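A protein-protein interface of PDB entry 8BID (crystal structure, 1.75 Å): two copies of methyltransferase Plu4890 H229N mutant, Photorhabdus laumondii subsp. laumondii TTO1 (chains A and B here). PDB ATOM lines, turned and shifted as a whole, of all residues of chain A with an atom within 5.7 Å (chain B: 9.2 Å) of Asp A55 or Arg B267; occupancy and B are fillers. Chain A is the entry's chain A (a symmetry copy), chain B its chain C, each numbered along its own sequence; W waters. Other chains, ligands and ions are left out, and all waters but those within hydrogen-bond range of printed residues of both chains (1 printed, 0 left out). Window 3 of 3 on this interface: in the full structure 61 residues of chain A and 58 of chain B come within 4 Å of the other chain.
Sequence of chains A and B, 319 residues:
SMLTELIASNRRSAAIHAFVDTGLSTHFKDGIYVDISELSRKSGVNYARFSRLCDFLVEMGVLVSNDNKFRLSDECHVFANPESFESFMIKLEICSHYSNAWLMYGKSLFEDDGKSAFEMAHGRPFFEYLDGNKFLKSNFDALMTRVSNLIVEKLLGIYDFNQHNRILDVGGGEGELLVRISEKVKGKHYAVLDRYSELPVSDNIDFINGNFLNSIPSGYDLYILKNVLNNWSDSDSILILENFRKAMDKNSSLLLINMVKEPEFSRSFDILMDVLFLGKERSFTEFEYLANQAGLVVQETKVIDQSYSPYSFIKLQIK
OG of Ser B266 is in hydrogen-bond range of N of Ser B268 (3.1 Å).
The side-chain carboxylate (OD2) of Asp B270 lies within salt-bridge range of the guanidinium group (NH1) of Arg B267 (2.9 Å).
OD1 of Asp B270 sits at hydrogen-bond distance from N of Glu B281, 3.0 Å away.
Ile B271 touches Arg A52 (CD1 to O, 3.6 Å).
Arg A52 touches Asp B274.
Arg A52 touches Lys B280.
Tyr B105 touches Leu A53 (OH to CB, 3.4 Å).
CD1 of Ile B271 touches N of Leu A53, 3.8 Å away.
Phe A56 touches Ser B266.
CZ of Phe A56 touches CB of Ser B268 (3.6 Å).
Phe A56 touches Ile B271.
Hydrophobic or aromatic side chains of chain B within 4 Å of the printed part of chain A: Tyr B105 and Ile B271.
Of the 12 printed residues of chain A, 5 touch a printed residue of chain B.
Hydrophobic or aromatic side chains of chain A that line the printed part of chain B: Leu A53 and Phe A56.
Among the printed residues, 13 pairs touch across the chains.
Of chain A, only Arg A52 (3.3 Å), Asp A55 (2.7 Å) and Glu A59 (2.8 Å) come within 4 Å of Arg B267.
No residue of chain B comes within 4 Å of Cys A54.
No residue of chain B comes within 4 Å of Val A58.
Of the printed residues of chain B, Arg A52 touches Arg B267, Asp B270, Ile B271, Asp B274 and Lys B280.
Printed residues of chain B within 4 Å of Glu A59: Ser B266 (2.7 Å) and Arg B267 (2.8 Å).
Of the printed residues of chain A, Lys B280 touches Arg A52.
Of the printed residues of chain A, Tyr B105 touches Leu A53.
Printed residues of chain A within 4 Å of Ser B268: Phe A56.
Glu B286 touches none of the printed residues of chain A.
The nearest residue of chain B that does not touch Asp A55 is Asp B270 (6.4 Å).
The nearest residue of chain A that does not touch Arg B267 is Phe A56 (4.03 Å).
The nearest printed residue of chain A that does not touch Asp B270 is Leu A53 (5.9 Å).
The side-chain carboxylate of Glu A59 sits at hydrogen-bond distance from the side-chain hydroxyl of Ser B266, at 2.7 Å.
O of Arg A52 is in hydrogen-bond range of NH1 of Arg B267 (3.3 Å).
The guanidinium group of Arg B267 lies within salt-bridge range of the side-chain carboxylate of Asp A55, at 2.7 Å.
The backbone NH of Arg B267 is in hydrogen-bond range of the side-chain carboxylate of Glu A59, 2.8 Å away.
The side-chain carboxylate (OD2) of Asp B270 lies within salt-bridge range of the guanidinium group (NE) of Arg A52 (2.7 Å).
Water W1 lies within hydrogen-bond range of OD1 of Asp B274 (2.6 Å) and NH1 of Arg A52 (2.9 Å).
No position is printed for both chains.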
ATOM      1  N   PHE A  50     -27.830 -19.331   4.316  1.00  0.00           N
ATOM      2  CA  PHE A  50     -28.601 -19.727   5.523  1.00  0.00           C
ATOM      3  C   PHE A  50     -28.359 -21.210   5.847  1.00  0.00           C
ATOM      4  O   PHE A  50     -28.354 -21.552   7.045  1.00  0.00           O
ATOM      5  CB  PHE A  50     -30.096 -19.443   5.386  1.00  0.00           C
ATOM      6  CG  PHE A  50     -30.855 -19.722   6.658  1.00  0.00           C
ATOM      7  CD1 PHE A  50     -30.465 -19.138   7.854  1.00  0.00           C
ATOM      8  CD2 PHE A  50     -31.929 -20.597   6.673  1.00  0.00           C
ATOM      9  CE1 PHE A  50     -31.140 -19.412   9.033  1.00  0.00           C
ATOM     10  CE2 PHE A  50     -32.616 -20.855   7.849  1.00  0.00           C
ATOM     11  CZ  PHE A  50     -32.218 -20.264   9.027  1.00  0.00           C
ATOM     12  N   SER A  51     -28.147 -22.066   4.839  1.00  0.00           N
ATOM     13  CA  SER A  51     -27.795 -23.498   5.054  1.00  0.00           C
ATOM     14  C   SER A  51     -26.489 -23.572   5.853  1.00  0.00           C
ATOM     15  O   SER A  51     -26.390 -24.406   6.766  1.00  0.00           O
ATOM     16  CB  SER A  51     -27.708 -24.270   3.765  1.00  0.00           C
ATOM     17  OG  SER A  51     -28.997 -24.389   3.179  1.00  0.00           O
ATOM     18  N   ARG A  52     -25.541 -22.693   5.556  1.00  0.00           N
ATOM     19  CA  ARG A  52     -24.220 -22.659   6.250  1.00  0.00           C
ATOM     20  C   ARG A  52     -24.405 -22.230   7.710  1.00  0.00           C
ATOM     21  O   ARG A  52     -23.750 -22.846   8.600  1.00  0.00           O
ATOM     22  CB  ARG A  52     -23.242 -21.781   5.467  1.00  0.00           C
ATOM     23  CG  ARG A  52     -22.592 -22.510   4.299  1.00  0.00           C
ATOM     24  CD  ARG A  52     -21.992 -21.576   3.264  1.00  0.00           C
ATOM     25  NE  ARG A  52     -21.001 -20.689   3.853  1.00  0.00           N
ATOM     26  CZ  ARG A  52     -20.609 -19.528   3.328  1.00  0.00           C
ATOM     27  NH1 ARG A  52     -21.118 -19.111   2.178  1.00  0.00           N
ATOM     28  NH2 ARG A  52     -19.708 -18.789   3.961  1.00  0.00           N
ATOM     29  N   LEU A  53     -25.253 -21.234   7.974  1.00  0.00           N
ATOM     30  CA  LEU A  53     -25.562 -20.796   9.365  1.00  0.00           C
ATOM     31  C   LEU A  53     -26.225 -21.953  10.122  1.00  0.00           C
ATOM     32  O   LEU A  53     -25.841 -22.205  11.258  1.00  0.00           O
ATOM     33  CB  LEU A  53     -26.457 -19.557   9.349  1.00  0.00           C
ATOM     34  CG  LEU A  53     -26.966 -19.088  10.714  1.00  0.00           C
ATOM     35  CD1 LEU A  53     -25.826 -18.820  11.676  1.00  0.00           C
ATOM     36  CD2 LEU A  53     -27.822 -17.842  10.563  1.00  0.00           C
ATOM     37  N   CYS A  54     -27.168 -22.657   9.499  1.00  0.00           N
ATOM     38  CA  CYS A  54     -27.865 -23.817  10.120  1.00  0.00           C
ATOM     39  C   CYS A  54     -26.830 -24.876  10.557  1.00  0.00           C
ATOM     40  O   CYS A  54     -26.967 -25.388  11.686  1.00  0.00           O
ATOM     41  CB  CYS A  54     -28.922 -24.396   9.185  1.00  0.00           C
ATOM     42  SG  CYS A  54     -30.425 -23.384   9.067  1.00  0.00           S
ATOM     43  N   ASP A  55     -25.814 -25.166   9.729  1.00  0.00           N
ATOM     44  CA  ASP A  55     -24.722 -26.135  10.047  1.00  0.00           C
ATOM     45  C   ASP A  55     -23.998 -25.703  11.334  1.00  0.00           C
ATOM     46  O   ASP A  55     -23.729 -26.573  12.187  1.00  0.00           O
ATOM     47  CB  ASP A  55     -23.734 -26.291   8.883  1.00  0.00           C
ATOM     48  CG  ASP A  55     -24.292 -26.943   7.622  1.00  0.00           C
ATOM     49  OD1 ASP A  55     -25.348 -27.619   7.703  1.00  0.00           O
ATOM     50  OD2 ASP A  55     -23.651 -26.781   6.550  1.00  0.00           O
ATOM     51  N   PHE A  56     -23.700 -24.415  11.491  1.00  0.00           N
ATOM     52  CA  PHE A  56     -23.015 -23.858  12.691  1.00  0.00           C
ATOM     53  C   PHE A  56     -23.967 -23.945  13.896  1.00  0.00           C
ATOM     54  O   PHE A  56     -23.506 -24.200  15.028  1.00  0.00           O
ATOM     55  CB  PHE A  56     -22.527 -22.431  12.420  1.00  0.00           C
ATOM     56  CG  PHE A  56     -21.705 -21.782  13.515  1.00  0.00           C
ATOM     57  CD1 PHE A  56     -20.795 -22.513  14.263  1.00  0.00           C
ATOM     58  CD2 PHE A  56     -21.830 -20.425  13.786  1.00  0.00           C
ATOM     59  CE1 PHE A  56     -20.023 -21.902  15.241  1.00  0.00           C
ATOM     60  CE2 PHE A  56     -21.063 -19.815  14.771  1.00  0.00           C
ATOM     61  CZ  PHE A  56     -20.161 -20.557  15.500  1.00  0.00           C
ATOM     62  N   LEU A  57     -25.271 -23.776  13.673  1.00  0.00           N
ATOM     63  CA  LEU A  57     -26.288 -23.885  14.759  1.00  0.00           C
ATOM     64  C   LEU A  57     -26.407 -25.350  15.203  1.00  0.00           C
ATOM     65  O   LEU A  57     -26.617 -25.580  16.420  1.00  0.00           O
ATOM     66  CB  LEU A  57     -27.630 -23.304  14.301  1.00  0.00           C
ATOM     67  CG  LEU A  57     -27.684 -21.779  14.145  1.00  0.00           C
ATOM     68  CD1 LEU A  57     -28.973 -21.350  13.453  1.00  0.00           C
ATOM     69  CD2 LEU A  57     -27.544 -21.070  15.487  1.00  0.00           C
ATOM     70  N   VAL A  58     -26.259 -26.310  14.281  1.00  0.00           N
ATOM     71  CA  VAL A  58     -26.223 -27.763  14.635  1.00  0.00           C
ATOM     72  C   VAL A  58     -24.986 -28.007  15.510  1.00  0.00           C
ATOM     73  O   VAL A  58     -25.139 -28.568  16.605  1.00  0.00           O
ATOM     74  CB  VAL A  58     -26.268 -28.684  13.399  1.00  0.00           C
ATOM     75  CG1 VAL A  58     -26.067 -30.142  13.776  1.00  0.00           C
ATOM     76  CG2 VAL A  58     -27.572 -28.524  12.623  1.00  0.00           C
ATOM     77  N   GLU A  59     -23.812 -27.554  15.077  1.00  0.00           N
ATOM     78  CA  GLU A  59     -22.549 -27.652  15.865  1.00  0.00           C
ATOM     79  C   GLU A  59     -22.773 -27.125  17.290  1.00  0.00           C
ATOM     80  O   GLU A  59     -22.313 -27.792  18.240  1.00  0.00           O
ATOM     81  CB  GLU A  59     -21.425 -26.902  15.151  1.00  0.00           C
ATOM     82  CG  GLU A  59     -20.158 -26.747  15.980  1.00  0.00           C
ATOM     83  CD  GLU A  59     -19.117 -25.890  15.282  1.00  0.00           C
ATOM     84  OE1 GLU A  59     -18.376 -25.159  15.975  1.00  0.00           O
ATOM     85  OE2 GLU A  59     -19.071 -25.943  14.044  1.00  0.00           O
ATOM     86  N   MET A  60     -23.453 -25.985  17.434  1.00  0.00           N
ATOM     87  CA  MET A  60     -23.745 -25.326  18.742  1.00  0.00           C
ATOM     88  C   MET A  60     -24.801 -26.103  19.542  1.00  0.00           C
ATOM     89  O   MET A  60     -24.931 -25.823  20.754  1.00  0.00           O
ATOM     90  CB  MET A  60     -24.257 -23.896  18.536  1.00  0.00           C
ATOM     91  CG  MET A  60     -23.162 -22.860  18.335  1.00  0.00           C
ATOM     92  SD  MET A  60     -23.844 -21.223  17.945  1.00  0.00           S
ATOM     93  CE  MET A  60     -23.903 -21.327  16.163  1.00  0.00           C
ATOM     94  N   PHE A  70     -34.230 -29.409   9.498  1.00  0.00           N
ATOM     95  CA  PHE A  70     -33.707 -28.936  10.807  1.00  0.00           C
ATOM     96  C   PHE A  70     -34.875 -28.608  11.736  1.00  0.00           C
ATOM     97  O   PHE A  70     -35.853 -27.977  11.280  1.00  0.00           O
ATOM     98  CB  PHE A  70     -32.810 -27.704  10.645  1.00  0.00           C
ATOM     99  CG  PHE A  70     -31.611 -27.892   9.749  1.00  0.00           C
ATOM    100  CD1 PHE A  70     -30.366 -28.205  10.269  1.00  0.00           C
ATOM    101  CD2 PHE A  70     -31.725 -27.728   8.382  1.00  0.00           C
ATOM    102  CE1 PHE A  70     -29.273 -28.370   9.434  1.00  0.00           C
ATOM    103  CE2 PHE A  70     -30.634 -27.899   7.547  1.00  0.00           C
ATOM    104  CZ  PHE A  70     -29.405 -28.212   8.076  1.00  0.00           C
ATOM    105  N   TRP B 102     -21.310  -7.916  12.248  1.00  0.00           N
ATOM    106  CA  TRP B 102     -22.114  -9.042  12.798  1.00  0.00           C
ATOM    107  C   TRP B 102     -23.572  -8.608  12.991  1.00  0.00           C
ATOM    108  O   TRP B 102     -24.440  -9.443  12.749  1.00  0.00           O
ATOM    109  CB  TRP B 102     -21.517  -9.605  14.094  1.00  0.00           C
ATOM    110  CG  TRP B 102     -20.404 -10.581  13.877  1.00  0.00           C
ATOM    111  CD1 TRP B 102     -19.080 -10.362  14.115  1.00  0.00           C
ATOM    112  CD2 TRP B 102     -20.503 -11.934  13.382  1.00  0.00           C
ATOM    113  NE1 TRP B 102     -18.352 -11.476  13.802  1.00  0.00           N
ATOM    114  CE2 TRP B 102     -19.190 -12.457  13.352  1.00  0.00           C
ATOM    115  CE3 TRP B 102     -21.558 -12.752  12.957  1.00  0.00           C
ATOM    116  CZ2 TRP B 102     -18.906 -13.758  12.938  1.00  0.00           C
ATOM    117  CZ3 TRP B 102     -21.282 -14.040  12.553  1.00  0.00           C
ATOM    118  CH2 TRP B 102     -19.972 -14.530  12.533  1.00  0.00           C
ATOM    119  N   TYR B 105     -25.494  -9.109   9.797  1.00  0.00           N
ATOM    120  CA  TYR B 105     -25.412 -10.494   9.260  1.00  0.00           C
ATOM    121  C   TYR B 105     -26.827 -11.007   8.939  1.00  0.00           C
ATOM    122  O   TYR B 105     -27.046 -11.430   7.803  1.00  0.00           O
ATOM    123  CB  TYR B 105     -24.654 -11.402  10.228  1.00  0.00           C
ATOM    124  CG  TYR B 105     -24.585 -12.859   9.832  1.00  0.00           C
ATOM    125  CD1 TYR B 105     -24.343 -13.255   8.525  1.00  0.00           C
ATOM    126  CD2 TYR B 105     -24.720 -13.849  10.791  1.00  0.00           C
ATOM    127  CE1 TYR B 105     -24.276 -14.594   8.178  1.00  0.00           C
ATOM    128  CE2 TYR B 105     -24.650 -15.192  10.462  1.00  0.00           C
ATOM    129  CZ  TYR B 105     -24.437 -15.569   9.149  1.00  0.00           C
ATOM    130  OH  TYR B 105     -24.389 -16.901   8.840  1.00  0.00           O
ATOM    131  N   VAL B 260      -8.433 -25.087   5.481  1.00  0.00           N
ATOM    132  CA  VAL B 260      -9.373 -26.006   4.772  1.00  0.00           C
ATOM    133  C   VAL B 260     -10.460 -26.450   5.759  1.00  0.00           C
ATOM    134  O   VAL B 260     -10.150 -26.622   6.966  1.00  0.00           O
ATOM    135  CB  VAL B 260      -8.624 -27.185   4.119  1.00  0.00           C
ATOM    136  CG1 VAL B 260      -7.878 -28.038   5.138  1.00  0.00           C
ATOM    137  CG2 VAL B 260      -9.549 -28.043   3.263  1.00  0.00           C
ATOM    138  N   LYS B 261     -11.690 -26.582   5.257  1.00  0.00           N
ATOM    139  CA  LYS B 261     -12.885 -27.009   6.029  1.00  0.00           C
ATOM    140  C   LYS B 261     -12.885 -28.538   6.094  1.00  0.00           C
ATOM    141  O   LYS B 261     -12.956 -29.176   5.018  1.00  0.00           O
ATOM    142  CB  LYS B 261     -14.158 -26.465   5.372  1.00  0.00           C
ATOM    143  CG  LYS B 261     -15.454 -26.700   6.141  1.00  0.00           C
ATOM    144  CD  LYS B 261     -16.642 -25.932   5.575  1.00  0.00           C
ATOM    145  CE  LYS B 261     -16.997 -26.289   4.142  1.00  0.00           C
ATOM    146  NZ  LYS B 261     -17.562 -27.655   4.030  1.00  0.00           N
ATOM    147  N   GLU B 262     -12.754 -29.091   7.305  1.00  0.00           N
ATOM    148  CA  GLU B 262     -12.908 -30.541   7.597  1.00  0.00           C
ATOM    149  C   GLU B 262     -14.034 -30.711   8.612  1.00  0.00           C
ATOM    150  O   GLU B 262     -14.219 -29.850   9.468  1.00  0.00           O
ATOM    151  CB  GLU B 262     -11.580 -31.120   8.080  1.00  0.00           C
ATOM    152  CG  GLU B 262     -10.529 -31.129   6.985  1.00  0.00           C
ATOM    153  CD  GLU B 262      -9.244 -31.868   7.305  1.00  0.00           C
ATOM    154  OE1 GLU B 262      -8.399 -31.998   6.391  1.00  0.00           O
ATOM    155  OE2 GLU B 262      -9.088 -32.306   8.466  1.00  0.00           O
ATOM    156  N   PRO B 263     -14.830 -31.806   8.533  1.00  0.00           N
ATOM    157  CA  PRO B 263     -16.007 -31.973   9.391  1.00  0.00           C
ATOM    158  C   PRO B 263     -15.715 -31.959  10.902  1.00  0.00           C
ATOM    159  O   PRO B 263     -16.598 -31.593  11.648  1.00  0.00           O
ATOM    160  CB  PRO B 263     -16.577 -33.344   8.984  1.00  0.00           C
ATOM    161  CG  PRO B 263     -16.027 -33.587   7.592  1.00  0.00           C
ATOM    162  CD  PRO B 263     -14.662 -32.926   7.590  1.00  0.00           C
ATOM    163  N   GLU B 264     -14.500 -32.335  11.314  1.00  0.00           N
ATOM    164  CA  GLU B 264     -14.103 -32.450  12.746  1.00  0.00           C
ATOM    165  C   GLU B 264     -13.997 -31.060  13.395  1.00  0.00           C
ATOM    166  O   GLU B 264     -14.083 -30.999  14.633  1.00  0.00           O
ATOM    167  CB  GLU B 264     -12.767 -33.185  12.901  1.00  0.00           C
ATOM    168  CG  GLU B 264     -12.800 -34.638  12.455  1.00  0.00           C
ATOM    169  CD  GLU B 264     -12.632 -34.879  10.961  1.00  0.00           C
ATOM    170  OE1 GLU B 264     -12.330 -33.912  10.226  1.00  0.00           O
ATOM    171  OE2 GLU B 264     -12.812 -36.038  10.533  1.00  0.00           O
ATOM    172  N   PHE B 265     -13.813 -29.992  12.608  1.00  0.00           N
ATOM    173  CA  PHE B 265     -13.468 -28.631  13.109  1.00  0.00           C
ATOM    174  C   PHE B 265     -14.658 -27.676  12.955  1.00  0.00           C
ATOM    175  O   PHE B 265     -15.596 -27.972  12.179  1.00  0.00           O
ATOM    176  CB  PHE B 265     -12.225 -28.102  12.389  1.00  0.00           C
ATOM    177  CG  PHE B 265     -10.969 -28.895  12.647  1.00  0.00           C
ATOM    178  CD1 PHE B 265     -10.061 -28.501  13.621  1.00  0.00           C
ATOM    179  CD2 PHE B 265     -10.696 -30.042  11.915  1.00  0.00           C
ATOM    180  CE1 PHE B 265      -8.906 -29.236  13.851  1.00  0.00           C
ATOM    181  CE2 PHE B 265      -9.545 -30.777  12.152  1.00  0.00           C
ATOM    182  CZ  PHE B 265      -8.652 -30.373  13.117  1.00  0.00           C
ATOM    183  N   SER B 266     -14.599 -26.543  13.663  1.00  0.00           N
ATOM    184  CA  SER B 266     -15.712 -25.566  13.820  1.00  0.00           C
ATOM    185  C   SER B 266     -16.068 -24.899  12.485  1.00  0.00           C
ATOM    186  O   SER B 266     -15.155 -24.643  11.668  1.00  0.00           O
ATOM    187  CB  SER B 266     -15.379 -24.531  14.860  1.00  0.00           C
ATOM    188  OG  SER B 266     -16.407 -23.552  14.954  1.00  0.00           O
ATOM    189  N   ARG B 267     -17.362 -24.618  12.284  1.00  0.00           N
ATOM    190  CA  ARG B 267     -17.874 -23.856  11.113  1.00  0.00           C
ATOM    191  C   ARG B 267     -17.788 -22.346  11.376  1.00  0.00           C
ATOM    192  O   ARG B 267     -18.198 -21.586  10.492  1.00  0.00           O
ATOM    193  CB  ARG B 267     -19.320 -24.266  10.806  1.00  0.00           C
ATOM    194  CG  ARG B 267     -19.440 -25.672  10.241  1.00  0.00           C
ATOM    195  CD  ARG B 267     -18.794 -25.767   8.871  1.00  0.00           C
ATOM    196  NE  ARG B 267     -19.748 -25.953   7.782  1.00  0.00           N
ATOM    197  CZ  ARG B 267     -20.599 -25.039   7.305  1.00  0.00           C
ATOM    198  NH1 ARG B 267     -20.682 -23.813   7.813  1.00  0.00           N
ATOM    199  NH2 ARG B 267     -21.388 -25.382   6.303  1.00  0.00           N
ATOM    200  N   SER B 268     -17.263 -21.908  12.525  1.00  0.00           N
ATOM    201  CA  SER B 268     -17.292 -20.477  12.934  1.00  0.00           C
ATOM    202  C   SER B 268     -16.540 -19.612  11.913  1.00  0.00           C
ATOM    203  O   SER B 268     -17.001 -18.476  11.634  1.00  0.00           O
ATOM    204  CB  SER B 268     -16.760 -20.287  14.321  1.00  0.00           C
ATOM    205  OG  SER B 268     -15.355 -20.171  14.306  1.00  0.00           O
ATOM    206  N   PHE B 269     -15.436 -20.120  11.358  1.00  0.00           N
ATOM    207  CA  PHE B 269     -14.594 -19.366  10.390  1.00  0.00           C
ATOM    208  C   PHE B 269     -15.373 -19.173   9.084  1.00  0.00           C
ATOM    209  O   PHE B 269     -15.352 -18.052   8.538  1.00  0.00           O
ATOM    210  CB  PHE B 269     -13.244 -20.041  10.151  1.00  0.00           C
ATOM    211  CG  PHE B 269     -12.274 -19.209   9.349  1.00  0.00           C
ATOM    212  CD1 PHE B 269     -11.592 -18.148   9.939  1.00  0.00           C
ATOM    213  CD2 PHE B 269     -12.036 -19.482   8.012  1.00  0.00           C
ATOM    214  CE1 PHE B 269     -10.710 -17.374   9.203  1.00  0.00           C
ATOM    215  CE2 PHE B 269     -11.151 -18.707   7.275  1.00  0.00           C
ATOM    216  CZ  PHE B 269     -10.486 -17.659   7.873  1.00  0.00           C
ATOM    217  N   ASP B 270     -16.049 -20.223   8.610  1.00  0.00           N
ATOM    218  CA  ASP B 270     -16.894 -20.171   7.387  1.00  0.00           C
ATOM    219  C   ASP B 270     -17.861 -18.986   7.501  1.00  0.00           C
ATOM    220  O   ASP B 270     -17.967 -18.210   6.531  1.00  0.00           O
ATOM    221  CB  ASP B 270     -17.616 -21.500   7.153  1.00  0.00           C
ATOM    222  CG  ASP B 270     -18.464 -21.511   5.895  1.00  0.00           C
ATOM    223  OD1 ASP B 270     -17.911 -21.258   4.815  1.00  0.00           O
ATOM    224  OD2 ASP B 270     -19.671 -21.743   6.010  1.00  0.00           O
ATOM    225  N   ILE B 271     -18.524 -18.846   8.652  1.00  0.00           N
ATOM    226  CA  ILE B 271     -19.528 -17.778   8.917  1.00  0.00           C
ATOM    227  C   ILE B 271     -18.811 -16.420   8.949  1.00  0.00           C
ATOM    228  O   ILE B 271     -19.326 -15.486   8.321  1.00  0.00           O
ATOM    229  CB  ILE B 271     -20.329 -18.090  10.200  1.00  0.00           C
ATOM    230  CG1 ILE B 271     -20.964 -19.489  10.169  1.00  0.00           C
ATOM    231  CG2 ILE B 271     -21.361 -17.003  10.471  1.00  0.00           C
ATOM    232  CD1 ILE B 271     -21.837 -19.787   8.948  1.00  0.00           C
ATOM    233  N   LEU B 272     -17.637 -16.300   9.586  1.00  0.00           N
ATOM    234  CA  LEU B 272     -16.899 -15.015   9.594  1.00  0.00           C
ATOM    235  C   LEU B 272     -16.614 -14.579   8.150  1.00  0.00           C
ATOM    236  O   LEU B 272     -16.731 -13.375   7.867  1.00  0.00           O
ATOM    237  CB  LEU B 272     -15.592 -15.145  10.379  1.00  0.00           C
ATOM    238  CG  LEU B 272     -14.829 -13.839  10.560  1.00  0.00           C
ATOM    239  CD1 LEU B 272     -15.620 -12.873  11.422  1.00  0.00           C
ATOM    240  CD2 LEU B 272     -13.447 -14.092  11.162  1.00  0.00           C
ATOM    241  N   MET B 273     -16.230 -15.513   7.272  1.00  0.00           N
ATOM    242  CA  MET B 273     -15.886 -15.195   5.868  1.00  0.00           C
ATOM    243  C   MET B 273     -17.144 -14.677   5.162  1.00  0.00           C
ATOM    244  O   MET B 273     -17.003 -13.721   4.361  1.00  0.00           O
ATOM    245  CB  MET B 273     -15.312 -16.403   5.121  1.00  0.00           C
ATOM    246  CG  MET B 273     -13.957 -16.888   5.636  1.00  0.00           C
ATOM    247  SD  MET B 273     -12.639 -15.627   5.692  1.00  0.00           S
ATOM    248  CE  MET B 273     -12.834 -15.017   7.366  1.00  0.00           C
ATOM    249  N   ASP B 274     -18.324 -15.241   5.465  1.00  0.00           N
ATOM    250  CA  ASP B 274     -19.620 -14.751   4.923  1.00  0.00           C
ATOM    251  C   ASP B 274     -19.822 -13.297   5.374  1.00  0.00           C
ATOM    252  O   ASP B 274     -20.062 -12.430   4.504  1.00  0.00           O
ATOM    253  CB  ASP B 274     -20.795 -15.628   5.356  1.00  0.00           C
ATOM    254  CG  ASP B 274     -22.080 -15.309   4.617  1.00  0.00           C
ATOM    255  OD1 ASP B 274     -22.028 -15.167   3.383  1.00  0.00           O
ATOM    256  OD2 ASP B 274     -23.111 -15.175   5.281  1.00  0.00           O
ATOM    257  N   LYS B 280     -16.115 -17.849   1.863  1.00  0.00           N
ATOM    258  CA  LYS B 280     -16.424 -19.143   2.529  1.00  0.00           C
ATOM    259  C   LYS B 280     -15.134 -19.929   2.748  1.00  0.00           C
ATOM    260  O   LYS B 280     -14.195 -19.746   1.952  1.00  0.00           O
ATOM    261  CB  LYS B 280     -17.434 -19.949   1.702  1.00  0.00           C
ATOM    262  CG  LYS B 280     -17.017 -20.283   0.280  1.00  0.00           C
ATOM    263  CD  LYS B 280     -18.079 -21.059  -0.510  1.00  0.00           C
ATOM    264  CE  LYS B 280     -19.227 -20.187  -0.975  1.00  0.00           C
ATOM    265  NZ  LYS B 280     -19.932 -20.762  -2.150  1.00  0.00           N
ATOM    266  N   GLU B 281     -15.097 -20.763   3.791  1.00  0.00           N
ATOM    267  CA  GLU B 281     -14.020 -21.768   3.986  1.00  0.00           C
ATOM    268  C   GLU B 281     -14.378 -23.008   3.172  1.00  0.00           C
ATOM    269  O   GLU B 281     -15.459 -23.557   3.393  1.00  0.00           O
ATOM    270  CB  GLU B 281     -13.814 -22.147   5.452  1.00  0.00           C
ATOM    271  CG  GLU B 281     -12.503 -22.888   5.658  1.00  0.00           C
ATOM    272  CD  GLU B 281     -12.215 -23.372   7.069  1.00  0.00           C
ATOM    273  OE1 GLU B 281     -11.041 -23.691   7.352  1.00  0.00           O
ATOM    274  OE2 GLU B 281     -13.161 -23.446   7.868  1.00  0.00           O
ATOM    275  N   ARG B 282     -13.490 -23.430   2.270  1.00  0.00           N
ATOM    276  CA  ARG B 282     -13.786 -24.497   1.279  1.00  0.00           C
ATOM    277  C   ARG B 282     -13.070 -25.795   1.675  1.00  0.00           C
ATOM    278  O   ARG B 282     -12.046 -25.723   2.412  1.00  0.00           O
ATOM    279  CB  ARG B 282     -13.419 -24.008  -0.123  1.00  0.00           C
ATOM    280  CG  ARG B 282     -14.290 -22.853  -0.596  1.00  0.00           C
ATOM    281  CD  ARG B 282     -13.996 -22.470  -2.029  1.00  0.00           C
ATOM    282  NE  ARG B 282     -14.812 -21.362  -2.510  1.00  0.00           N
ATOM    283  CZ  ARG B 282     -14.550 -20.070  -2.328  1.00  0.00           C
ATOM    284  NH1 ARG B 282     -13.484 -19.680  -1.643  1.00  0.00           N
ATOM    285  NH2 ARG B 282     -15.364 -19.167  -2.842  1.00  0.00           N
ATOM    286  N   SER B 283     -13.625 -26.929   1.230  1.00  0.00           N
ATOM    287  CA  SER B 283     -13.021 -28.285   1.302  1.00  0.00           C
ATOM    288  C   SER B 283     -12.012 -28.446   0.162  1.00  0.00           C
ATOM    289  O   SER B 283     -12.047 -27.618  -0.777  1.00  0.00           O
ATOM    290  CB  SER B 283     -14.084 -29.348   1.221  1.00  0.00           C
ATOM    291  OG  SER B 283     -14.813 -29.231   0.005  1.00  0.00           O
ATOM    292  N   GLU B 286     -14.009 -28.665  -3.124  1.00  0.00           N
ATOM    293  CA  GLU B 286     -14.512 -27.346  -3.602  1.00  0.00           C
ATOM    294  C   GLU B 286     -13.375 -26.558  -4.277  1.00  0.00           C
ATOM    295  O   GLU B 286     -13.619 -25.994  -5.362  1.00  0.00           O
ATOM    296  CB  GLU B 286     -15.165 -26.590  -2.443  1.00  0.00           C
ATOM    297  CG  GLU B 286     -16.544 -27.132  -2.090  1.00  0.00           C
ATOM    298  CD  GLU B 286     -17.182 -26.580  -0.827  1.00  0.00           C
ATOM    299  OE1 GLU B 286     -16.449 -26.121   0.069  1.00  0.00           O
ATOM    300  OE2 GLU B 286     -18.420 -26.618  -0.740  1.00  0.00           O
HETATM  301  O   HOH W   1     -20.765 -16.310   1.427  1.00  0.00           O
